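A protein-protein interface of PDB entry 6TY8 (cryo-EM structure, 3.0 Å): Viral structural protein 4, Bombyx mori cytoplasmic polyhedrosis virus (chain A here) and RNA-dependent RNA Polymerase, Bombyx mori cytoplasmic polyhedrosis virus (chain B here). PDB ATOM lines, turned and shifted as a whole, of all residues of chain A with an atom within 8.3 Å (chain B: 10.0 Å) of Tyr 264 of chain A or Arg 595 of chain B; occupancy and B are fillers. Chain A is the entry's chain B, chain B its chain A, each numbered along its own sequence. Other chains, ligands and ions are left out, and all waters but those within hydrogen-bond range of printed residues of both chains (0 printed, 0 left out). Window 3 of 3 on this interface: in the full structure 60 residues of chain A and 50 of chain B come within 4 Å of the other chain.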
ATOM      1  N   THR A 261       2.477  21.781  25.478  1.00  0.00           N
ATOM      2  CA  THR A 261       2.734  21.113  24.214  1.00  0.00           C
ATOM      3  C   THR A 261       1.444  20.493  23.697  1.00  0.00           C
ATOM      4  O   THR A 261       0.444  20.393  24.408  1.00  0.00           O
ATOM      5  CB  THR A 261       3.800  20.029  24.366  1.00  0.00           C
ATOM      6  OG1 THR A 261       3.341  19.040  25.288  1.00  0.00           O
ATOM      7  CG2 THR A 261       5.076  20.610  24.887  1.00  0.00           C
ATOM      8  N   GLY A 262       1.467  20.060  22.444  1.00  0.00           N
ATOM      9  CA  GLY A 262       0.264  19.490  21.878  1.00  0.00           C
ATOM     10  C   GLY A 262       0.577  18.531  20.755  1.00  0.00           C
ATOM     11  O   GLY A 262       1.720  18.384  20.323  1.00  0.00           O
ATOM     12  N   ILE A 263      -0.480  17.863  20.296  1.00  0.00           N
ATOM     13  CA  ILE A 263      -0.365  16.964  19.156  1.00  0.00           C
ATOM     14  C   ILE A 263      -0.168  17.773  17.888  1.00  0.00           C
ATOM     15  O   ILE A 263       0.512  17.346  16.950  1.00  0.00           O
ATOM     16  CB  ILE A 263      -1.615  16.070  19.068  1.00  0.00           C
ATOM     17  CG1 ILE A 263      -1.933  15.461  20.433  1.00  0.00           C
ATOM     18  CG2 ILE A 263      -1.418  14.955  18.068  1.00  0.00           C
ATOM     19  CD1 ILE A 263      -0.842  14.586  21.003  1.00  0.00           C
ATOM     20  N   TYR A 264      -0.729  18.977  17.859  1.00  0.00           N
ATOM     21  CA  TYR A 264      -0.809  19.793  16.661  1.00  0.00           C
ATOM     22  C   TYR A 264       0.103  21.007  16.719  1.00  0.00           C
ATOM     23  O   TYR A 264       0.335  21.636  15.685  1.00  0.00           O
ATOM     24  CB  TYR A 264      -2.257  20.246  16.450  1.00  0.00           C
ATOM     25  CG  TYR A 264      -3.233  19.109  16.246  1.00  0.00           C
ATOM     26  CD1 TYR A 264      -2.826  17.901  15.696  1.00  0.00           C
ATOM     27  CD2 TYR A 264      -4.542  19.216  16.680  1.00  0.00           C
ATOM     28  CE1 TYR A 264      -3.702  16.860  15.538  1.00  0.00           C
ATOM     29  CE2 TYR A 264      -5.426  18.177  16.529  1.00  0.00           C
ATOM     30  CZ  TYR A 264      -4.998  17.002  15.956  1.00  0.00           C
ATOM     31  OH  TYR A 264      -5.868  15.954  15.800  1.00  0.00           O
ATOM     32  N   GLY A 265       0.616  21.352  17.888  1.00  0.00           N
ATOM     33  CA  GLY A 265       1.447  22.528  18.032  1.00  0.00           C
ATOM     34  C   GLY A 265       1.540  22.941  19.485  1.00  0.00           C
ATOM     35  O   GLY A 265       1.542  22.107  20.380  1.00  0.00           O
ATOM     36  N   GLU A 266       1.642  24.249  19.684  1.00  0.00           N
ATOM     37  CA  GLU A 266       1.758  24.839  21.010  1.00  0.00           C
ATOM     38  C   GLU A 266       0.435  25.468  21.428  1.00  0.00           C
ATOM     39  O   GLU A 266      -0.132  26.290  20.704  1.00  0.00           O
ATOM     40  CB  GLU A 266       2.889  25.868  21.003  1.00  0.00           C
ATOM     41  CG  GLU A 266       3.174  26.609  22.289  1.00  0.00           C
ATOM     42  CD  GLU A 266       2.525  27.983  22.314  1.00  0.00           C
ATOM     43  OE1 GLU A 266       2.287  28.541  21.223  1.00  0.00           O
ATOM     44  OE2 GLU A 266       2.286  28.523  23.412  1.00  0.00           O
ATOM     45  N   VAL A 267      -0.057  25.074  22.603  1.00  0.00           N
ATOM     46  CA  VAL A 267      -1.399  25.422  23.064  1.00  0.00           C
ATOM     47  C   VAL A 267      -1.293  26.228  24.349  1.00  0.00           C
ATOM     48  O   VAL A 267      -0.604  25.819  25.287  1.00  0.00           O
ATOM     49  CB  VAL A 267      -2.258  24.161  23.296  1.00  0.00           C
ATOM     50  CG1 VAL A 267      -3.643  24.533  23.779  1.00  0.00           C
ATOM     51  CG2 VAL A 267      -2.347  23.340  22.036  1.00  0.00           C
ATOM     52  N   ILE A 299      -8.892  27.021  27.286  1.00  0.00           N
ATOM     53  CA  ILE A 299      -7.968  27.000  26.157  1.00  0.00           C
ATOM     54  C   ILE A 299      -8.323  28.146  25.218  1.00  0.00           C
ATOM     55  O   ILE A 299      -9.483  28.284  24.810  1.00  0.00           O
ATOM     56  CB  ILE A 299      -8.024  25.651  25.424  1.00  0.00           C
ATOM     57  CG1 ILE A 299      -7.489  24.538  26.312  1.00  0.00           C
ATOM     58  CG2 ILE A 299      -7.241  25.698  24.128  1.00  0.00           C
ATOM     59  CD1 ILE A 299      -7.782  23.172  25.777  1.00  0.00           C
ATOM     60  N   THR A 300      -7.334  28.972  24.878  1.00  0.00           N
ATOM     61  CA  THR A 300      -7.549  30.116  24.002  1.00  0.00           C
ATOM     62  C   THR A 300      -7.200  29.834  22.546  1.00  0.00           C
ATOM     63  O   THR A 300      -6.961  30.779  21.787  1.00  0.00           O
ATOM     64  CB  THR A 300      -6.749  31.326  24.490  1.00  0.00           C
ATOM     65  OG1 THR A 300      -5.357  30.998  24.537  1.00  0.00           O
ATOM     66  CG2 THR A 300      -7.204  31.740  25.856  1.00  0.00           C
ATOM     67  N   ASP A 301      -7.165  28.574  22.136  1.00  0.00           N
ATOM     68  CA  ASP A 301      -6.911  28.229  20.748  1.00  0.00           C
ATOM     69  C   ASP A 301      -8.130  27.569  20.118  1.00  0.00           C
ATOM     70  O   ASP A 301      -9.061  27.148  20.808  1.00  0.00           O
ATOM     71  CB  ASP A 301      -5.699  27.309  20.628  1.00  0.00           C
ATOM     72  CG  ASP A 301      -4.398  28.035  20.875  1.00  0.00           C
ATOM     73  OD1 ASP A 301      -4.339  29.257  20.624  1.00  0.00           O
ATOM     74  OD2 ASP A 301      -3.428  27.385  21.304  1.00  0.00           O
ATOM     75  N   ALA A 302      -8.107  27.483  18.790  1.00  0.00           N
ATOM     76  CA  ALA A 302      -9.235  26.960  18.038  1.00  0.00           C
ATOM     77  C   ALA A 302      -9.392  25.467  18.258  1.00  0.00           C
ATOM     78  O   ALA A 302      -8.432  24.705  18.141  1.00  0.00           O
ATOM     79  CB  ALA A 302      -9.049  27.234  16.547  1.00  0.00           C
ATOM     80  N   ILE A 303     -10.611  25.049  18.580  1.00  0.00           N
ATOM     81  CA  ILE A 303     -10.904  23.624  18.664  1.00  0.00           C
ATOM     82  C   ILE A 303     -10.977  23.088  17.239  1.00  0.00           C
ATOM     83  O   ILE A 303     -11.497  23.774  16.345  1.00  0.00           O
ATOM     84  CB  ILE A 303     -12.180  23.351  19.480  1.00  0.00           C
ATOM     85  CG1 ILE A 303     -13.391  24.089  18.917  1.00  0.00           C
ATOM     86  CG2 ILE A 303     -11.972  23.741  20.929  1.00  0.00           C
ATOM     87  CD1 ILE A 303     -14.694  23.677  19.545  1.00  0.00           C
ATOM     88  N   PRO A 304     -10.415  21.907  16.951  1.00  0.00           N
ATOM     89  CA  PRO A 304      -9.663  20.979  17.804  1.00  0.00           C
ATOM     90  C   PRO A 304      -8.244  21.419  18.164  1.00  0.00           C
ATOM     91  O   PRO A 304      -7.427  21.709  17.295  1.00  0.00           O
ATOM     92  CB  PRO A 304      -9.612  19.711  16.958  1.00  0.00           C
ATOM     93  CG  PRO A 304      -9.705  20.190  15.565  1.00  0.00           C
ATOM     94  CD  PRO A 304     -10.599  21.373  15.593  1.00  0.00           C
ATOM     95  N   SER A 305      -7.968  21.476  19.460  1.00  0.00           N
ATOM     96  CA  SER A 305      -6.630  21.765  19.945  1.00  0.00           C
ATOM     97  C   SER A 305      -5.941  20.477  20.365  1.00  0.00           C
ATOM     98  O   SER A 305      -6.587  19.478  20.669  1.00  0.00           O
ATOM     99  CB  SER A 305      -6.691  22.727  21.122  1.00  0.00           C
ATOM    100  OG  SER A 305      -7.341  22.122  22.221  1.00  0.00           O
ATOM    101  N   GLY A 306      -4.619  20.509  20.414  1.00  0.00           N
ATOM    102  CA  GLY A 306      -3.884  19.280  20.637  1.00  0.00           C
ATOM    103  C   GLY A 306      -3.667  18.868  22.080  1.00  0.00           C
ATOM    104  O   GLY A 306      -2.711  18.149  22.372  1.00  0.00           O
ATOM    105  N   ILE A 307      -4.542  19.299  22.987  1.00  0.00           N
ATOM    106  CA  ILE A 307      -4.398  18.953  24.397  1.00  0.00           C
ATOM    107  C   ILE A 307      -4.765  17.492  24.611  1.00  0.00           C
ATOM    108  O   ILE A 307      -5.881  17.062  24.303  1.00  0.00           O
ATOM    109  CB  ILE A 307      -5.246  19.877  25.275  1.00  0.00           C
ATOM    110  CG1 ILE A 307      -4.632  21.266  25.293  1.00  0.00           C
ATOM    111  CG2 ILE A 307      -5.337  19.344  26.679  1.00  0.00           C
ATOM    112  CD1 ILE A 307      -3.264  21.285  25.902  1.00  0.00           C
ATOM    113  N   SER A 308      -3.820  16.725  25.143  1.00  0.00           N
ATOM    114  CA  SER A 308      -4.007  15.321  25.455  1.00  0.00           C
ATOM    115  C   SER A 308      -3.478  15.058  26.856  1.00  0.00           C
ATOM    116  O   SER A 308      -2.989  15.957  27.539  1.00  0.00           O
ATOM    117  CB  SER A 308      -3.309  14.434  24.420  1.00  0.00           C
ATOM    118  OG  SER A 308      -1.911  14.654  24.431  1.00  0.00           O
ATOM    119  N   SER A 311       0.421  15.926  27.421  1.00  0.00           N
ATOM    120  CA  SER A 311       0.985  17.242  27.162  1.00  0.00           C
ATOM    121  C   SER A 311       1.770  17.735  28.368  1.00  0.00           C
ATOM    122  O   SER A 311       1.343  17.597  29.515  1.00  0.00           O
ATOM    123  CB  SER A 311      -0.116  18.241  26.824  1.00  0.00           C
ATOM    124  OG  SER A 311      -0.762  17.900  25.615  1.00  0.00           O
ATOM    125  N   GLU A 438     -10.674   5.947  11.600  1.00  0.00           N
ATOM    126  CA  GLU A 438      -9.979   7.152  11.157  1.00  0.00           C
ATOM    127  C   GLU A 438      -9.706   7.166   9.658  1.00  0.00           C
ATOM    128  O   GLU A 438      -9.494   8.243   9.091  1.00  0.00           O
ATOM    129  CB  GLU A 438      -8.645   7.299  11.894  1.00  0.00           C
ATOM    130  CG  GLU A 438      -8.743   7.700  13.349  1.00  0.00           C
ATOM    131  CD  GLU A 438      -9.166   9.136  13.520  1.00  0.00           C
ATOM    132  OE1 GLU A 438      -8.823   9.959  12.644  1.00  0.00           O
ATOM    133  OE2 GLU A 438      -9.833   9.451  14.528  1.00  0.00           O
ATOM    134  N   ASP A 512      -9.899  18.179  24.281  1.00  0.00           N
ATOM    135  CA  ASP A 512     -10.191  17.818  22.907  1.00  0.00           C
ATOM    136  C   ASP A 512     -10.924  16.492  23.003  1.00  0.00           C
ATOM    137  O   ASP A 512     -10.318  15.472  23.342  1.00  0.00           O
ATOM    138  CB  ASP A 512      -8.936  17.703  22.052  1.00  0.00           C
ATOM    139  CG  ASP A 512      -9.250  17.722  20.571  1.00  0.00           C
ATOM    140  OD1 ASP A 512     -10.423  17.973  20.233  1.00  0.00           O
ATOM    141  OD2 ASP A 512      -8.352  17.454  19.750  1.00  0.00           O
ATOM    142  N   THR A 514     -12.340  14.638  20.702  1.00  0.00           N
ATOM    143  CA  THR A 514     -11.865  13.683  19.712  1.00  0.00           C
ATOM    144  C   THR A 514     -10.475  13.161  20.028  1.00  0.00           C
ATOM    145  O   THR A 514     -10.029  12.210  19.383  1.00  0.00           O
ATOM    146  CB  THR A 514     -11.854  14.310  18.320  1.00  0.00           C
ATOM    147  OG1 THR A 514     -11.533  13.307  17.349  1.00  0.00           O
ATOM    148  CG2 THR A 514     -10.825  15.394  18.244  1.00  0.00           C
ATOM    149  N   GLN A 515      -9.778  13.763  20.986  1.00  0.00           N
ATOM    150  CA  GLN A 515      -8.521  13.217  21.461  1.00  0.00           C
ATOM    151  C   GLN A 515      -8.713  12.326  22.673  1.00  0.00           C
ATOM    152  O   GLN A 515      -8.038  11.299  22.777  1.00  0.00           O
ATOM    153  CB  GLN A 515      -7.551  14.345  21.805  1.00  0.00           C
ATOM    154  CG  GLN A 515      -6.149  13.903  22.106  1.00  0.00           C
ATOM    155  CD  GLN A 515      -5.454  13.356  20.889  1.00  0.00           C
ATOM    156  OE1 GLN A 515      -5.586  13.901  19.794  1.00  0.00           O
ATOM    157  NE2 GLN A 515      -4.711  12.271  21.065  1.00  0.00           N
ATOM    158  N   ARG A 518     -10.106   9.175  21.555  1.00  0.00           N
ATOM    159  CA  ARG A 518      -9.087   8.438  20.819  1.00  0.00           C
ATOM    160  C   ARG A 518      -8.014   7.886  21.750  1.00  0.00           C
ATOM    161  O   ARG A 518      -7.481   6.801  21.502  1.00  0.00           O
ATOM    162  CB  ARG A 518      -8.461   9.353  19.765  1.00  0.00           C
ATOM    163  CG  ARG A 518      -7.508   8.693  18.799  1.00  0.00           C
ATOM    164  CD  ARG A 518      -6.947   9.713  17.824  1.00  0.00           C
ATOM    165  NE  ARG A 518      -7.965  10.271  16.938  1.00  0.00           N
ATOM    166  CZ  ARG A 518      -7.767  11.318  16.142  1.00  0.00           C
ATOM    167  NH1 ARG A 518      -6.590  11.925  16.124  1.00  0.00           N
ATOM    168  NH2 ARG A 518      -8.746  11.765  15.368  1.00  0.00           N
ATOM    169  N   HIS B 378     -16.576  30.364  20.648  1.00  0.00           N
ATOM    170  CA  HIS B 378     -16.920  29.371  19.630  1.00  0.00           C
ATOM    171  C   HIS B 378     -18.368  29.482  19.170  1.00  0.00           C
ATOM    172  O   HIS B 378     -18.939  28.514  18.663  1.00  0.00           O
ATOM    173  CB  HIS B 378     -16.601  27.957  20.107  1.00  0.00           C
ATOM    174  CG  HIS B 378     -15.168  27.775  20.487  1.00  0.00           C
ATOM    175  ND1 HIS B 378     -14.712  27.971  21.771  1.00  0.00           N
ATOM    176  CD2 HIS B 378     -14.083  27.460  19.747  1.00  0.00           C
ATOM    177  CE1 HIS B 378     -13.409  27.761  21.812  1.00  0.00           C
ATOM    178  NE2 HIS B 378     -13.004  27.448  20.595  1.00  0.00           N
ATOM    179  N   VAL B 589     -11.080  35.962  15.997  1.00  0.00           N
ATOM    180  CA  VAL B 589     -11.943  35.081  15.218  1.00  0.00           C
ATOM    181  C   VAL B 589     -11.186  33.796  14.921  1.00  0.00           C
ATOM    182  O   VAL B 589     -10.065  33.834  14.408  1.00  0.00           O
ATOM    183  CB  VAL B 589     -12.396  35.778  13.912  1.00  0.00           C
ATOM    184  CG1 VAL B 589     -12.872  34.787  12.920  1.00  0.00           C
ATOM    185  CG2 VAL B 589     -13.529  36.758  14.170  1.00  0.00           C
ATOM    186  N   PHE B 590     -11.784  32.656  15.253  1.00  0.00           N
ATOM    187  CA  PHE B 590     -11.246  31.372  14.835  1.00  0.00           C
ATOM    188  C   PHE B 590     -11.832  31.023  13.476  1.00  0.00           C
ATOM    189  O   PHE B 590     -12.971  31.379  13.175  1.00  0.00           O
ATOM    190  CB  PHE B 590     -11.574  30.254  15.822  1.00  0.00           C
ATOM    191  CG  PHE B 590     -11.114  30.507  17.227  1.00  0.00           C
ATOM    192  CD1 PHE B 590      -9.771  30.556  17.540  1.00  0.00           C
ATOM    193  CD2 PHE B 590     -12.032  30.611  18.247  1.00  0.00           C
ATOM    194  CE1 PHE B 590      -9.359  30.761  18.838  1.00  0.00           C
ATOM    195  CE2 PHE B 590     -11.622  30.811  19.539  1.00  0.00           C
ATOM    196  CZ  PHE B 590     -10.287  30.888  19.835  1.00  0.00           C
ATOM    197  N   GLU B 591     -11.051  30.338  12.647  1.00  0.00           N
ATOM    198  CA  GLU B 591     -11.496  29.946  11.319  1.00  0.00           C
ATOM    199  C   GLU B 591     -11.202  28.469  11.095  1.00  0.00           C
ATOM    200  O   GLU B 591     -10.728  27.764  11.987  1.00  0.00           O
ATOM    201  CB  GLU B 591     -10.831  30.798  10.234  1.00  0.00           C
ATOM    202  CG  GLU B 591     -11.227  32.257  10.298  1.00  0.00           C
ATOM    203  CD  GLU B 591     -10.579  33.089   9.228  1.00  0.00           C
ATOM    204  OE1 GLU B 591      -9.764  32.549   8.459  1.00  0.00           O
ATOM    205  OE2 GLU B 591     -10.877  34.295   9.168  1.00  0.00           O
ATOM    206  N   VAL B 592     -11.492  28.001   9.887  1.00  0.00           N
ATOM    207  CA  VAL B 592     -11.272  26.601   9.540  1.00  0.00           C
ATOM    208  C   VAL B 592      -9.934  26.450   8.832  1.00  0.00           C
ATOM    209  O   VAL B 592      -9.663  27.124   7.833  1.00  0.00           O
ATOM    210  CB  VAL B 592     -12.424  26.068   8.681  1.00  0.00           C
ATOM    211  CG1 VAL B 592     -12.040  24.758   8.014  1.00  0.00           C
ATOM    212  CG2 VAL B 592     -13.620  25.836   9.557  1.00  0.00           C
ATOM    213  N   GLY B 593      -9.096  25.553   9.347  1.00  0.00           N
ATOM    214  CA  GLY B 593      -7.749  25.376   8.874  1.00  0.00           C
ATOM    215  C   GLY B 593      -6.737  26.232   9.596  1.00  0.00           C
ATOM    216  O   GLY B 593      -5.535  25.962   9.508  1.00  0.00           O
ATOM    217  N   LYS B 594      -7.195  27.254  10.304  1.00  0.00           N
ATOM    218  CA  LYS B 594      -6.337  28.131  11.078  1.00  0.00           C
ATOM    219  C   LYS B 594      -6.256  27.596  12.498  1.00  0.00           C
ATOM    220  O   LYS B 594      -7.285  27.411  13.156  1.00  0.00           O
ATOM    221  CB  LYS B 594      -6.879  29.561  11.078  1.00  0.00           C
ATOM    222  CG  LYS B 594      -6.334  30.484   9.993  1.00  0.00           C
ATOM    223  CD  LYS B 594      -6.691  30.033   8.590  1.00  0.00           C
ATOM    224  CE  LYS B 594      -6.098  30.962   7.549  1.00  0.00           C
ATOM    225  NZ  LYS B 594      -6.663  32.336   7.657  1.00  0.00           N
ATOM    226  N   ARG B 595      -5.041  27.348  12.966  1.00  0.00           N
ATOM    227  CA  ARG B 595      -4.820  26.794  14.293  1.00  0.00           C
ATOM    228  C   ARG B 595      -4.878  27.860  15.382  1.00  0.00           C
ATOM    229  O   ARG B 595      -5.082  27.527  16.553  1.00  0.00           O
ATOM    230  CB  ARG B 595      -3.468  26.070  14.300  1.00  0.00           C
ATOM    231  CG  ARG B 595      -3.150  25.185  15.483  1.00  0.00           C
ATOM    232  CD  ARG B 595      -1.782  24.585  15.267  1.00  0.00           C
ATOM    233  NE  ARG B 595      -0.779  25.640  15.206  1.00  0.00           N
ATOM    234  CZ  ARG B 595       0.466  25.472  14.777  1.00  0.00           C
ATOM    235  NH1 ARG B 595       0.872  24.282  14.359  1.00  0.00           N
ATOM    236  NH2 ARG B 595       1.304  26.500  14.758  1.00  0.00           N
ATOM    237  N   GLN B 596      -4.732  29.133  15.019  1.00  0.00           N
ATOM    238  CA  GLN B 596      -4.845  30.239  15.956  1.00  0.00           C
ATOM    239  C   GLN B 596      -5.974  31.170  15.542  1.00  0.00           C
ATOM    240  O   GLN B 596      -6.650  30.956  14.535  1.00  0.00           O
ATOM    241  CB  GLN B 596      -3.541  31.027  16.049  1.00  0.00           C
ATOM    242  CG  GLN B 596      -2.420  30.263  16.698  1.00  0.00           C
ATOM    243  CD  GLN B 596      -1.172  31.093  16.816  1.00  0.00           C
ATOM    244  OE1 GLN B 596      -1.124  32.230  16.350  1.00  0.00           O
ATOM    245  NE2 GLN B 596      -0.149  30.536  17.451  1.00  0.00           N
ATOM    246  N   SER B 597      -6.167  32.215  16.342  1.00  0.00           N
ATOM    247  CA  SER B 597      -7.275  33.134  16.125  1.00  0.00           C
ATOM    248  C   SER B 597      -6.875  34.255  15.175  1.00  0.00           C
ATOM    249  O   SER B 597      -5.856  34.922  15.373  1.00  0.00           O
ATOM    250  CB  SER B 597      -7.741  33.719  17.454  1.00  0.00           C
ATOM    251  OG  SER B 597      -6.755  34.566  18.005  1.00  0.00           O
ATOM    252  N   GLN B 598      -7.690  34.469  14.146  1.00  0.00           N
ATOM    253  CA  GLN B 598      -7.505  35.578  13.227  1.00  0.00           C
ATOM    254  C   GLN B 598      -8.157  36.826  13.815  1.00  0.00           C
ATOM    255  O   GLN B 598      -8.715  36.801  14.910  1.00  0.00           O
ATOM    256  CB  GLN B 598      -8.101  35.228  11.869  1.00  0.00           C
ATOM    257  CG  GLN B 598      -7.515  33.978  11.247  1.00  0.00           C
ATOM    258  CD  GLN B 598      -6.041  34.106  10.968  1.00  0.00           C
ATOM    259  OE1 GLN B 598      -5.216  33.474  11.623  1.00  0.00           O
ATOM    260  NE2 GLN B 598      -5.698  34.932   9.992  1.00  0.00           N
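Thr 300 of chain A touches Phe 590 of chain B (O to CE1, 3.8 Å). His 378 of chain B touches Asp 301 of chain A (NE2 to O, 3.96 Å). C of Asp 301 of chain A touches CE1 of Phe 590 of chain B (3.7 Å). Ala 302 of chain A touches Phe 590 of chain B (N to CE1, 3.5 Å). Lys 594 of chain B touches Ala 302 of chain A (O to CB, 3.8 Å). Ala 302 of chain A touches Arg 595 of chain B. CG1 of Ile 303 of chain A touches CD2 of His 378 of chain B, at 3.5 Å.
Of the 11 printed residues of chain B, 4 touch a printed residue of chain A. Of the 23 printed residues of chain A, 5 touch a printed residue of chain B. Hydrophobic or aromatic side chains of chain A within 4 Å of the printed part of chain B: Ala 302 and Ile 303.
The guanidinium group (NH1) of Arg 595 of chain B is in hydrogen-bond range of the backbone carbonyl oxygen (O) of Tyr 264 of chain A (3.0 Å).
OE1 of Glu 591 of chain B lies within salt-bridge range of NZ of Lys 594 of chain B (3.2 Å).
No residue of chain B comes within 4 Å of Gly 262 of chain A. No residue of chain B comes within 4 Å of Ile 263 of chain A. Tyr 264 of chain A touches just one residue of chain B: Arg 595. No residue of chain B comes within 4 Å of Gly 265 of chain A. Of the printed residues of chain B, Thr 300 of chain A touches Phe 590. Ala 302 of chain A touches just these residues of chain B: Phe 590, Lys 594 and Arg 595. No residue of chain B comes within 4 Å of Gly 306 of chain A. Of the printed residues of chain A, His 378 of chain B touches Asp 301 (3.96 Å) and Ile 303 (3.5 Å). Printed residues of chain A within 4 Å of Arg 595 of chain B: Tyr 264 (3.0 Å) and Ala 302 (3.8 Å). The nearest printed residue of chain A that does not touch Arg 595 of chain B is Gly 265 of chain A (4.1 Å).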
